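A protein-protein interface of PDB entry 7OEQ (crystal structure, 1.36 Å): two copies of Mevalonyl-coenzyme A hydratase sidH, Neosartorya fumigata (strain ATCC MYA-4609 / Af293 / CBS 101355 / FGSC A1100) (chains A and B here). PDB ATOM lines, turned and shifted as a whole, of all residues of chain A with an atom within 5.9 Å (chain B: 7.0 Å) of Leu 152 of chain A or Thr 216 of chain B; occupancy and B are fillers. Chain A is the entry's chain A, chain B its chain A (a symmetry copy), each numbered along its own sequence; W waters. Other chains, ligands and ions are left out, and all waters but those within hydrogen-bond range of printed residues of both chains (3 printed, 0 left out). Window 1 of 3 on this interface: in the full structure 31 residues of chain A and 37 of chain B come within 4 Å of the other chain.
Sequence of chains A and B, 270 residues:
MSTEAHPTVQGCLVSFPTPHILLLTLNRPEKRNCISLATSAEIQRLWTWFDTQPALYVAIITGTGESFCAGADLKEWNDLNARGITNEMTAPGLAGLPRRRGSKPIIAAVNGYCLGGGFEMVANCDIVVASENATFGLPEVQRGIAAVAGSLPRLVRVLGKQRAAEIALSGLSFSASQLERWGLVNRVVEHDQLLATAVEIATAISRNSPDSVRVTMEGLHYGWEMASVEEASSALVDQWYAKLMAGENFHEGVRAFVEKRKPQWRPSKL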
ATOM      1  N   GLU A 120       8.476  17.473  10.036  1.00  0.00           N
ATOM      2  CA  GLU A 120       7.863  17.620   8.682  1.00  0.00           C
ATOM      3  C   GLU A 120       6.983  18.887   8.581  1.00  0.00           C
ATOM      4  O   GLU A 120       7.002  19.559   7.525  1.00  0.00           O
ATOM      5  CB  GLU A 120       7.080  16.372   8.294  1.00  0.00           C
ATOM      6  CG  GLU A 120       7.919  15.097   8.324  1.00  0.00           C
ATOM      7  CD  GLU A 120       7.498  14.052   7.274  1.00  0.00           C
ATOM      8  OE1 GLU A 120       6.937  13.030   7.640  1.00  0.00           O
ATOM      9  OE2 GLU A 120       7.810  14.267   6.112  1.00  0.00           O
ATOM     10  N   LEU A 138      14.097  12.984  12.392  1.00  0.00           N
ATOM     11  CA  LEU A 138      13.082  12.099  11.751  1.00  0.00           C
ATOM     12  C   LEU A 138      13.320  10.670  12.208  1.00  0.00           C
ATOM     13  O   LEU A 138      13.947   9.887  11.507  1.00  0.00           O
ATOM     14  CB  LEU A 138      13.177  12.227  10.236  1.00  0.00           C
ATOM     15  CG  LEU A 138      12.848  13.586   9.626  1.00  0.00           C
ATOM     16  CD1 LEU A 138      13.160  13.548   8.126  1.00  0.00           C
ATOM     17  CD2 LEU A 138      11.403  13.995   9.915  1.00  0.00           C
ATOM     18  N   VAL A 141      12.641   6.123  10.626  1.00  0.00           N
ATOM     19  CA  VAL A 141      13.455   4.976  10.119  1.00  0.00           C
ATOM     20  C   VAL A 141      13.836   4.039  11.282  1.00  0.00           C
ATOM     21  O   VAL A 141      14.014   2.841  11.016  1.00  0.00           O
ATOM     22  CB  VAL A 141      14.719   5.415   9.366  1.00  0.00           C
ATOM     23  CG1 VAL A 141      14.428   5.942   7.990  1.00  0.00           C
ATOM     24  CG2 VAL A 141      15.591   6.376  10.192  1.00  0.00           C
ATOM     25  N   ILE A 145       9.001   2.773   9.952  1.00  0.00           N
ATOM     26  CA  ILE A 145       8.160   3.558   9.000  1.00  0.00           C
ATOM     27  C   ILE A 145       9.090   4.559   8.291  1.00  0.00           C
ATOM     28  O   ILE A 145      10.294   4.299   8.230  1.00  0.00           O
ATOM     29  CB  ILE A 145       6.913   4.157   9.696  1.00  0.00           C
ATOM     30  CG1 ILE A 145       5.709   4.290   8.753  1.00  0.00           C
ATOM     31  CG2 ILE A 145       7.213   5.463  10.415  1.00  0.00           C
ATOM     32  CD1 ILE A 145       4.454   4.822   9.424  1.00  0.00           C
ATOM     33  N   ALA A 146       8.565   5.608   7.688  1.00  0.00           N
ATOM     34  CA  ALA A 146       9.388   6.574   6.944  1.00  0.00           C
ATOM     35  C   ALA A 146       8.687   7.919   7.002  1.00  0.00           C
ATOM     36  O   ALA A 146       7.458   7.938   7.291  1.00  0.00           O
ATOM     37  CB  ALA A 146       9.613   6.100   5.532  1.00  0.00           C
ATOM     38  N   ALA A 147       9.447   8.986   6.775  1.00  0.00           N
ATOM     39  CA  ALA A 147       8.920  10.357   6.770  1.00  0.00           C
ATOM     40  C   ALA A 147       8.251  10.572   5.416  1.00  0.00           C
ATOM     41  O   ALA A 147       8.961  10.930   4.469  1.00  0.00           O
ATOM     42  CB  ALA A 147      10.045  11.328   7.059  1.00  0.00           C
ATOM     43  N   VAL A 148       6.941  10.353   5.335  1.00  0.00           N
ATOM     44  CA  VAL A 148       6.216  10.423   4.036  1.00  0.00           C
ATOM     45  C   VAL A 148       5.225  11.575   4.032  1.00  0.00           C
ATOM     46  O   VAL A 148       4.460  11.661   3.064  1.00  0.00           O
ATOM     47  CB  VAL A 148       5.528   9.097   3.682  1.00  0.00           C
ATOM     48  CG1 VAL A 148       6.520   7.962   3.593  1.00  0.00           C
ATOM     49  CG2 VAL A 148       4.439   8.755   4.675  1.00  0.00           C
ATOM     50  N   GLY A 150       5.834  14.689   3.344  1.00  0.00           N
ATOM     51  CA  GLY A 150       6.238  15.666   2.313  1.00  0.00           C
ATOM     52  C   GLY A 150       7.565  16.373   2.610  1.00  0.00           C
ATOM     53  O   GLY A 150       8.050  17.169   1.757  1.00  0.00           O
ATOM     54  N   SER A 151       8.201  16.098   3.744  1.00  0.00           N
ATOM     55  CA  SER A 151       9.446  16.786   4.099  1.00  0.00           C
ATOM     56  C   SER A 151      10.616  16.346   3.217  1.00  0.00           C
ATOM     57  O   SER A 151      11.550  17.177   3.051  1.00  0.00           O
ATOM     58  CB  SER A 151       9.809  16.664   5.578  1.00  0.00           C
ATOM     59  OG  SER A 151      10.217  15.347   5.902  1.00  0.00           O
ATOM     60  N   LEU A 152      10.696  15.091   2.776  1.00  0.00           N
ATOM     61  CA  LEU A 152      11.963  14.619   2.155  1.00  0.00           C
ATOM     62  C   LEU A 152      12.340  15.470   0.951  1.00  0.00           C
ATOM     63  O   LEU A 152      13.477  15.945   0.865  1.00  0.00           O
ATOM     64  CB  LEU A 152      11.989  13.124   1.864  1.00  0.00           C
ATOM     65  CG  LEU A 152      11.836  12.201   3.073  1.00  0.00           C
ATOM     66  CD1 LEU A 152      11.760  10.745   2.654  1.00  0.00           C
ATOM     67  CD2 LEU A 152      13.010  12.410   4.031  1.00  0.00           C
ATOM     68  N   PRO A 153      11.469  15.698  -0.058  1.00  0.00           N
ATOM     69  CA  PRO A 153      11.899  16.515  -1.198  1.00  0.00           C
ATOM     70  C   PRO A 153      12.175  17.982  -0.820  1.00  0.00           C
ATOM     71  O   PRO A 153      13.022  18.610  -1.432  1.00  0.00           O
ATOM     72  CB  PRO A 153      10.751  16.353  -2.208  1.00  0.00           C
ATOM     73  CG  PRO A 153       9.579  15.970  -1.374  1.00  0.00           C
ATOM     74  CD  PRO A 153      10.124  15.133  -0.233  1.00  0.00           C
ATOM     75  N   ARG A 154      11.450  18.486   0.173  1.00  0.00           N
ATOM     76  CA  ARG A 154      11.599  19.871   0.674  1.00  0.00           C
ATOM     77  C   ARG A 154      12.951  20.006   1.384  1.00  0.00           C
ATOM     78  O   ARG A 154      13.682  20.963   1.101  1.00  0.00           O
ATOM     79  CB  ARG A 154      10.403  20.244   1.554  1.00  0.00           C
ATOM     80  CG  ARG A 154       9.107  20.338   0.763  1.00  0.00           C
ATOM     81  CD  ARG A 154       7.895  20.549   1.654  1.00  0.00           C
ATOM     82  NE  ARG A 154       6.653  20.887   0.917  1.00  0.00           N
ATOM     83  CZ  ARG A 154       5.850  20.010   0.294  1.00  0.00           C
ATOM     84  NH1 ARG A 154       6.148  18.726   0.261  1.00  0.00           N
ATOM     85  NH2 ARG A 154       4.779  20.461  -0.317  1.00  0.00           N
ATOM     86  N   LEU A 155      13.309  19.035   2.198  1.00  0.00           N
ATOM     87  CA  LEU A 155      14.616  19.103   2.913  1.00  0.00           C
ATOM     88  C   LEU A 155      15.753  18.994   1.913  1.00  0.00           C
ATOM     89  O   LEU A 155      16.793  19.643   2.071  1.00  0.00           O
ATOM     90  CB  LEU A 155      14.698  18.018   3.986  1.00  0.00           C
ATOM     91  CG  LEU A 155      13.826  18.260   5.220  1.00  0.00           C
ATOM     92  CD1 LEU A 155      13.821  17.036   6.136  1.00  0.00           C
ATOM     93  CD2 LEU A 155      14.247  19.503   5.965  1.00  0.00           C
ATOM     94  N   VAL A 156      15.601  18.170   0.858  1.00  0.00           N
ATOM     95  CA  VAL A 156      16.637  18.088  -0.209  1.00  0.00           C
ATOM     96  C   VAL A 156      16.862  19.493  -0.774  1.00  0.00           C
ATOM     97  O   VAL A 156      18.018  19.871  -1.033  1.00  0.00           O
ATOM     98  CB  VAL A 156      16.248  17.063  -1.308  1.00  0.00           C
ATOM     99  CG1 VAL A 156      17.103  17.189  -2.558  1.00  0.00           C
ATOM    100  CG2 VAL A 156      16.364  15.670  -0.720  1.00  0.00           C
ATOM    101  N   ARG A 157      15.783  20.248  -1.003  1.00  0.00           N
ATOM    102  CA  ARG A 157      15.880  21.582  -1.626  1.00  0.00           C
ATOM    103  C   ARG A 157      16.365  22.669  -0.678  1.00  0.00           C
ATOM    104  O   ARG A 157      16.722  23.732  -1.208  1.00  0.00           O
ATOM    105  CB  ARG A 157      14.545  21.944  -2.265  1.00  0.00           C
ATOM    106  CG  ARG A 157      14.240  21.026  -3.447  1.00  0.00           C
ATOM    107  CD  ARG A 157      13.002  21.467  -4.075  1.00  0.00           C
ATOM    108  NE  ARG A 157      12.637  20.517  -5.109  1.00  0.00           N
ATOM    109  CZ  ARG A 157      12.093  20.874  -6.224  1.00  0.00           C
ATOM    110  NH1 ARG A 157      11.938  22.158  -6.501  1.00  0.00           N
ATOM    111  NH2 ARG A 157      11.774  19.944  -7.075  1.00  0.00           N
ATOM    112  N   ALA A 164      20.087  16.325   3.948  1.00  0.00           N
ATOM    113  CA  ALA A 164      18.768  15.674   4.086  1.00  0.00           C
ATOM    114  C   ALA A 164      18.967  14.159   4.291  1.00  0.00           C
ATOM    115  O   ALA A 164      18.279  13.562   5.129  1.00  0.00           O
ATOM    116  CB  ALA A 164      17.941  15.942   2.841  1.00  0.00           C
ATOM    117  N   ALA A 168      17.664  12.013   7.460  1.00  0.00           N
ATOM    118  CA  ALA A 168      16.545  11.088   7.237  1.00  0.00           C
ATOM    119  C   ALA A 168      17.000   9.627   7.326  1.00  0.00           C
ATOM    120  O   ALA A 168      16.215   8.798   7.808  1.00  0.00           O
ATOM    121  CB  ALA A 168      15.844  11.354   5.915  1.00  0.00           C
ATOM    122  N   LEU A 169      18.184   9.295   6.828  1.00  0.00           N
ATOM    123  CA  LEU A 169      18.661   7.890   6.862  1.00  0.00           C
ATOM    124  C   LEU A 169      19.092   7.459   8.264  1.00  0.00           C
ATOM    125  O   LEU A 169      18.951   6.275   8.589  1.00  0.00           O
ATOM    126  CB  LEU A 169      19.782   7.667   5.848  1.00  0.00           C
ATOM    127  CG  LEU A 169      19.405   7.930   4.398  1.00  0.00           C
ATOM    128  CD1 LEU A 169      20.657   7.997   3.547  1.00  0.00           C
ATOM    129  CD2 LEU A 169      18.434   6.861   3.855  1.00  0.00           C
ATOM    130  N   ASP B 211      13.676  -1.741   5.099  1.00  0.00           N
ATOM    131  CA  ASP B 211      12.551  -1.226   4.284  1.00  0.00           C
ATOM    132  C   ASP B 211      12.449   0.293   4.420  1.00  0.00           C
ATOM    133  O   ASP B 211      12.222   0.999   3.403  1.00  0.00           O
ATOM    134  CB  ASP B 211      11.208  -1.877   4.641  1.00  0.00           C
ATOM    135  CG  ASP B 211      11.080  -3.356   4.327  1.00  0.00           C
ATOM    136  OD1 ASP B 211      11.775  -3.822   3.423  1.00  0.00           O
ATOM    137  OD2 ASP B 211      10.255  -4.020   4.985  1.00  0.00           O
ATOM    138  N   SER B 212      12.506   0.796   5.645  1.00  0.00           N
ATOM    139  CA  SER B 212      12.469   2.247   5.913  1.00  0.00           C
ATOM    140  C   SER B 212      13.602   2.954   5.145  1.00  0.00           C
ATOM    141  O   SER B 212      13.395   4.044   4.607  1.00  0.00           O
ATOM    142  CB  SER B 212      12.577   2.520   7.400  1.00  0.00           C
ATOM    143  OG  SER B 212      11.521   1.939   8.176  1.00  0.00           O
ATOM    144  N   VAL B 213      14.800   2.389   5.138  1.00  0.00           N
ATOM    145  CA  VAL B 213      15.943   3.042   4.450  1.00  0.00           C
ATOM    146  C   VAL B 213      15.671   3.041   2.929  1.00  0.00           C
ATOM    147  O   VAL B 213      15.936   4.096   2.273  1.00  0.00           O
ATOM    148  CB  VAL B 213      17.267   2.368   4.841  1.00  0.00           C
ATOM    149  CG1 VAL B 213      18.406   2.832   3.957  1.00  0.00           C
ATOM    150  CG2 VAL B 213      17.596   2.624   6.307  1.00  0.00           C
ATOM    151  N   ARG B 214      15.102   1.955   2.367  1.00  0.00           N
ATOM    152  CA  ARG B 214      14.826   1.906   0.915  1.00  0.00           C
ATOM    153  C   ARG B 214      13.826   3.026   0.560  1.00  0.00           C
ATOM    154  O   ARG B 214      14.045   3.769  -0.443  1.00  0.00           O
ATOM    155  CB  ARG B 214      14.273   0.529   0.533  1.00  0.00           C
ATOM    156  CG  ARG B 214      15.306  -0.590   0.435  1.00  0.00           C
ATOM    157  CD  ARG B 214      16.196  -0.557  -0.798  1.00  0.00           C
ATOM    158  NE  ARG B 214      15.308  -0.588  -1.937  1.00  0.00           N
ATOM    159  CZ  ARG B 214      14.945   0.437  -2.713  1.00  0.00           C
ATOM    160  NH1 ARG B 214      14.048   0.214  -3.636  1.00  0.00           N
ATOM    161  NH2 ARG B 214      15.471   1.634  -2.636  1.00  0.00           N
ATOM    162  N   VAL B 215      12.727   3.125   1.320  1.00  0.00           N
ATOM    163  CA  VAL B 215      11.665   4.116   1.005  1.00  0.00           C
ATOM    164  C   VAL B 215      12.212   5.532   1.188  1.00  0.00           C
ATOM    165  O   VAL B 215      11.870   6.431   0.388  1.00  0.00           O
ATOM    166  CB  VAL B 215      10.405   3.869   1.848  1.00  0.00           C
ATOM    167  CG1 VAL B 215       9.387   4.983   1.697  1.00  0.00           C
ATOM    168  CG2 VAL B 215       9.811   2.519   1.486  1.00  0.00           C
ATOM    169  N   THR B 216      13.036   5.756   2.207  1.00  0.00           N
ATOM    170  CA  THR B 216      13.638   7.087   2.424  1.00  0.00           C
ATOM    171  C   THR B 216      14.524   7.445   1.217  1.00  0.00           C
ATOM    172  O   THR B 216      14.465   8.602   0.761  1.00  0.00           O
ATOM    173  CB  THR B 216      14.364   7.120   3.773  1.00  0.00           C
ATOM    174  OG1 THR B 216      13.462   6.789   4.824  1.00  0.00           O
ATOM    175  CG2 THR B 216      14.983   8.470   4.049  1.00  0.00           C
ATOM    176  N   MET B 217      15.339   6.504   0.720  1.00  0.00           N
ATOM    177  CA  MET B 217      16.191   6.754  -0.459  1.00  0.00           C
ATOM    178  C   MET B 217      15.296   7.194  -1.633  1.00  0.00           C
ATOM    179  O   MET B 217      15.628   8.172  -2.321  1.00  0.00           O
ATOM    180  CB  MET B 217      16.986   5.509  -0.847  1.00  0.00           C
ATOM    181  CG  MET B 217      18.163   5.162   0.045  1.00  0.00           C
ATOM    182  SD  MET B 217      19.495   6.381   0.040  1.00  0.00           S
ATOM    183  CE  MET B 217      20.067   6.139  -1.636  1.00  0.00           C
ATOM    184  N   GLU B 218      14.179   6.470  -1.854  1.00  0.00           N
ATOM    185  CA  GLU B 218      13.273   6.854  -2.963  1.00  0.00           C
ATOM    186  C   GLU B 218      12.792   8.298  -2.779  1.00  0.00           C
ATOM    187  O   GLU B 218      12.837   9.085  -3.747  1.00  0.00           O
ATOM    188  CB  GLU B 218      12.105   5.877  -3.120  1.00  0.00           C
ATOM    189  CG  GLU B 218      12.574   4.449  -3.349  1.00  0.00           C
ATOM    190  CD  GLU B 218      13.140   4.154  -4.725  1.00  0.00           C
ATOM    191  OE1 GLU B 218      12.897   4.958  -5.628  1.00  0.00           O
ATOM    192  OE2 GLU B 218      13.882   3.134  -4.868  1.00  0.00           O
ATOM    193  N   GLY B 219      12.343   8.648  -1.573  1.00  0.00           N
ATOM    194  CA  GLY B 219      11.797   9.986  -1.327  1.00  0.00           C
ATOM    195  C   GLY B 219      12.846  11.058  -1.566  1.00  0.00           C
ATOM    196  O   GLY B 219      12.497  12.144  -2.051  1.00  0.00           O
ATOM    197  N   LEU B 220      14.077  10.804  -1.139  1.00  0.00           N
ATOM    198  CA  LEU B 220      15.207  11.751  -1.348  1.00  0.00           C
ATOM    199  C   LEU B 220      15.498  11.899  -2.848  1.00  0.00           C
ATOM    200  O   LEU B 220      15.712  13.031  -3.334  1.00  0.00           O
ATOM    201  CB  LEU B 220      16.442  11.226  -0.600  1.00  0.00           C
ATOM    202  CG  LEU B 220      16.380  11.283   0.939  1.00  0.00           C
ATOM    203  CD1 LEU B 220      17.497  10.418   1.479  1.00  0.00           C
ATOM    204  CD2 LEU B 220      16.500  12.715   1.481  1.00  0.00           C
ATOM    205  N   HIS B 221      15.461  10.804  -3.596  1.00  0.00           N
ATOM    206  CA  HIS B 221      15.691  10.860  -5.067  1.00  0.00           C
ATOM    207  C   HIS B 221      14.643  11.741  -5.758  1.00  0.00           C
ATOM    208  O   HIS B 221      14.985  12.520  -6.663  1.00  0.00           O
ATOM    209  CB  HIS B 221      15.647   9.481  -5.728  1.00  0.00           C
ATOM    210  CG  HIS B 221      16.849   8.628  -5.500  1.00  0.00           C
ATOM    211  ND1 HIS B 221      18.129   9.110  -5.643  1.00  0.00           N
ATOM    212  CD2 HIS B 221      16.977   7.321  -5.165  1.00  0.00           C
ATOM    213  CE1 HIS B 221      18.995   8.146  -5.403  1.00  0.00           C
ATOM    214  NE2 HIS B 221      18.321   7.048  -5.068  1.00  0.00           N
ATOM    215  N   TYR B 222      13.393  11.642  -5.339  1.00  0.00           N
ATOM    216  CA  TYR B 222      12.295  12.311  -6.088  1.00  0.00           C
ATOM    217  C   TYR B 222      12.513  13.827  -6.047  1.00  0.00           C
ATOM    218  O   TYR B 222      12.114  14.511  -6.949  1.00  0.00           O
ATOM    219  CB  TYR B 222      10.926  11.928  -5.533  1.00  0.00           C
ATOM    220  CG  TYR B 222      10.498  10.505  -5.785  1.00  0.00           C
ATOM    221  CD1 TYR B 222      10.933   9.799  -6.904  1.00  0.00           C
ATOM    222  CD2 TYR B 222       9.623   9.865  -4.933  1.00  0.00           C
ATOM    223  CE1 TYR B 222      10.544   8.493  -7.148  1.00  0.00           C
ATOM    224  CE2 TYR B 222       9.183   8.571  -5.186  1.00  0.00           C
ATOM    225  CZ  TYR B 222       9.652   7.873  -6.285  1.00  0.00           C
ATOM    226  OH  TYR B 222       9.258   6.582  -6.513  1.00  0.00           O
ATOM    227  N   GLY B 223      13.165  14.316  -4.989  1.00  0.00           N
ATOM    228  CA  GLY B 223      13.606  15.717  -4.816  1.00  0.00           C
ATOM    229  C   GLY B 223      14.480  16.247  -5.951  1.00  0.00           C
ATOM    230  O   GLY B 223      14.381  17.464  -6.223  1.00  0.00           O
ATOM    231  N   ALA B 232       6.643  15.032  -6.089  1.00  0.00           N
ATOM    232  CA  ALA B 232       7.577  14.144  -5.357  1.00  0.00           C
ATOM    233  C   ALA B 232       6.881  13.579  -4.116  1.00  0.00           C
ATOM    234  O   ALA B 232       7.081  12.411  -3.810  1.00  0.00           O
ATOM    235  CB  ALA B 232       8.818  14.897  -4.988  1.00  0.00           C
ATOM    236  N   SER B 233       6.129  14.397  -3.398  1.00  0.00           N
ATOM    237  CA  SER B 233       5.407  13.966  -2.178  1.00  0.00           C
ATOM    238  C   SER B 233       4.357  12.897  -2.517  1.00  0.00           C
ATOM    239  O   SER B 233       4.271  11.897  -1.817  1.00  0.00           O
ATOM    240  CB  SER B 233       4.767  15.148  -1.469  1.00  0.00           C
ATOM    241  OG  SER B 233       5.775  16.099  -1.070  1.00  0.00           O
ATOM    242  N   LEU B 236       5.951   9.440  -3.634  1.00  0.00           N
ATOM    243  CA  LEU B 236       6.472   8.569  -2.576  1.00  0.00           C
ATOM    244  C   LEU B 236       5.323   7.794  -1.915  1.00  0.00           C
ATOM    245  O   LEU B 236       5.479   6.582  -1.701  1.00  0.00           O
ATOM    246  CB  LEU B 236       7.212   9.446  -1.575  1.00  0.00           C
ATOM    247  CG  LEU B 236       7.873   8.675  -0.445  1.00  0.00           C
ATOM    248  CD1 LEU B 236       8.904   7.694  -0.986  1.00  0.00           C
ATOM    249  CD2 LEU B 236       8.465   9.646   0.542  1.00  0.00           C
ATOM    250  N   LEU B 244       5.606  -0.534   2.165  1.00  0.00           N
ATOM    251  CA  LEU B 244       6.296  -0.401   3.478  1.00  0.00           C
ATOM    252  C   LEU B 244       5.423  -0.965   4.613  1.00  0.00           C
ATOM    253  O   LEU B 244       5.929  -1.763   5.424  1.00  0.00           O
ATOM    254  CB  LEU B 244       6.601   1.080   3.707  1.00  0.00           C
ATOM    255  CG  LEU B 244       7.313   1.418   5.010  1.00  0.00           C
ATOM    256  CD1 LEU B 244       8.657   0.698   5.112  1.00  0.00           C
ATOM    257  CD2 LEU B 244       7.498   2.924   5.143  1.00  0.00           C
HETATM  258  O   HOH W   1      12.256   8.609   6.541  1.00  0.00           O
HETATM  259  O   HOH W   2       5.532  12.068   0.663  1.00  0.00           O
HETATM  260  O   HOH W   3      10.821  17.385  -6.264  1.00  0.00           O
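The side-chain carboxylate (OE2) of Glu 120 of chain A lies within hydrogen-bond range of the backbone NH (N) of Gly 150 of chain A (3.4 Å). The guanidinium group (NH1) of Arg 154 of chain A lies within hydrogen-bond range of the backbone carbonyl oxygen (O) of Gly 150 of chain A (2.9 Å). The backbone carbonyl oxygen (O) of Ser 212 of chain B sits at hydrogen-bond distance from the side-chain hydroxyl (OG1) of Thr 216 of chain B (2.8 Å).
Water W2 lies within hydrogen-bond range of O of Val 148 of chain A (2.7 Å) and O of Ser 233 of chain B (2.8 Å). Water W1 lies within hydrogen-bond range of OG1 of Thr 216 of chain B (2.8 Å) and N of Ala 147 of chain A (2.8 Å). Water W3 bridges the guanidinium group of Arg 157 of chain A (2.8 Å) and the backbone carbonyl oxygen of Tyr 222 of chain B (3.2 Å).
Hydrophobic or aromatic side chains of chain A that line the printed part of chain B: Val 141, Ala 146, Val 148, Leu 152, Pro 153, Val 156, Ala 164, Ala 168 and Leu 169. Among the printed residues, 19 pairs touch across the chains.
OG of Ser 212 of chain B is in hydrogen-bond range of O of Ile 145 of chain A, at 2.7 Å. The side-chain hydroxyl (OG) of Ser 233 of chain B is in hydrogen-bond range of the guanidinium group (NH1) of Arg 154 of chain A (3.0 Å).
CG1 of Val 141 of chain A touches OG1 of Thr 216 of chain B (3.4 Å). Ile 145 of chain A touches Leu 244 of chain B. Ala 146 of chain A touches Thr 216 of chain B (CB to OG1, 3.97 Å). Gly 150 of chain A touches Ser 233 of chain B (CA to OG, 3.4 Å). O of Thr 216 of chain B touches CD1 of Leu 152 of chain A, 3.9 Å away. Pro 153 of chain A touches Ala 232 of chain B. CG of Pro 153 of chain A touches OG of Ser 233 of chain B, at 3.8 Å. CG2 of Val 156 of chain A touches CD2 of Leu 220 of chain B, 3.7 Å away. Leu 220 of chain B touches Ala 164 of chain A. CB of Ala 168 of chain A touches CG2 of Thr 216 of chain B, at 3.5 Å.
Leu 152 of chain A touches one residue of chain B. Of chain A, only Val 141 (3.4 Å), Ala 146 (3.97 Å), Leu 152 (3.9 Å), Ala 168 (3.5 Å) and Leu 169 (3.8 Å) come within 4 Å of Thr 216 of chain B. Printed residues of chain B within 4 Å of Pro 153 of chain A: Gly 223 (3.9 Å), Ala 232 (3.7 Å) and Ser 233 (3.8 Å). Printed residues of chain A within 4 Å of Ala 232 of chain B: Pro 153. Of the printed residues of chain A, Leu 220 of chain B touches Val 156 (3.7 Å) and Ala 164 (3.8 Å). The nearest residue of chain A that does not touch Thr 216 of chain B is Ala 147 of chain A (5.0 Å).
No position is printed for both chains. Of the 19 pairs that touch across the chains among the printed residues, none has its exchanged pair printed and touching as well.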
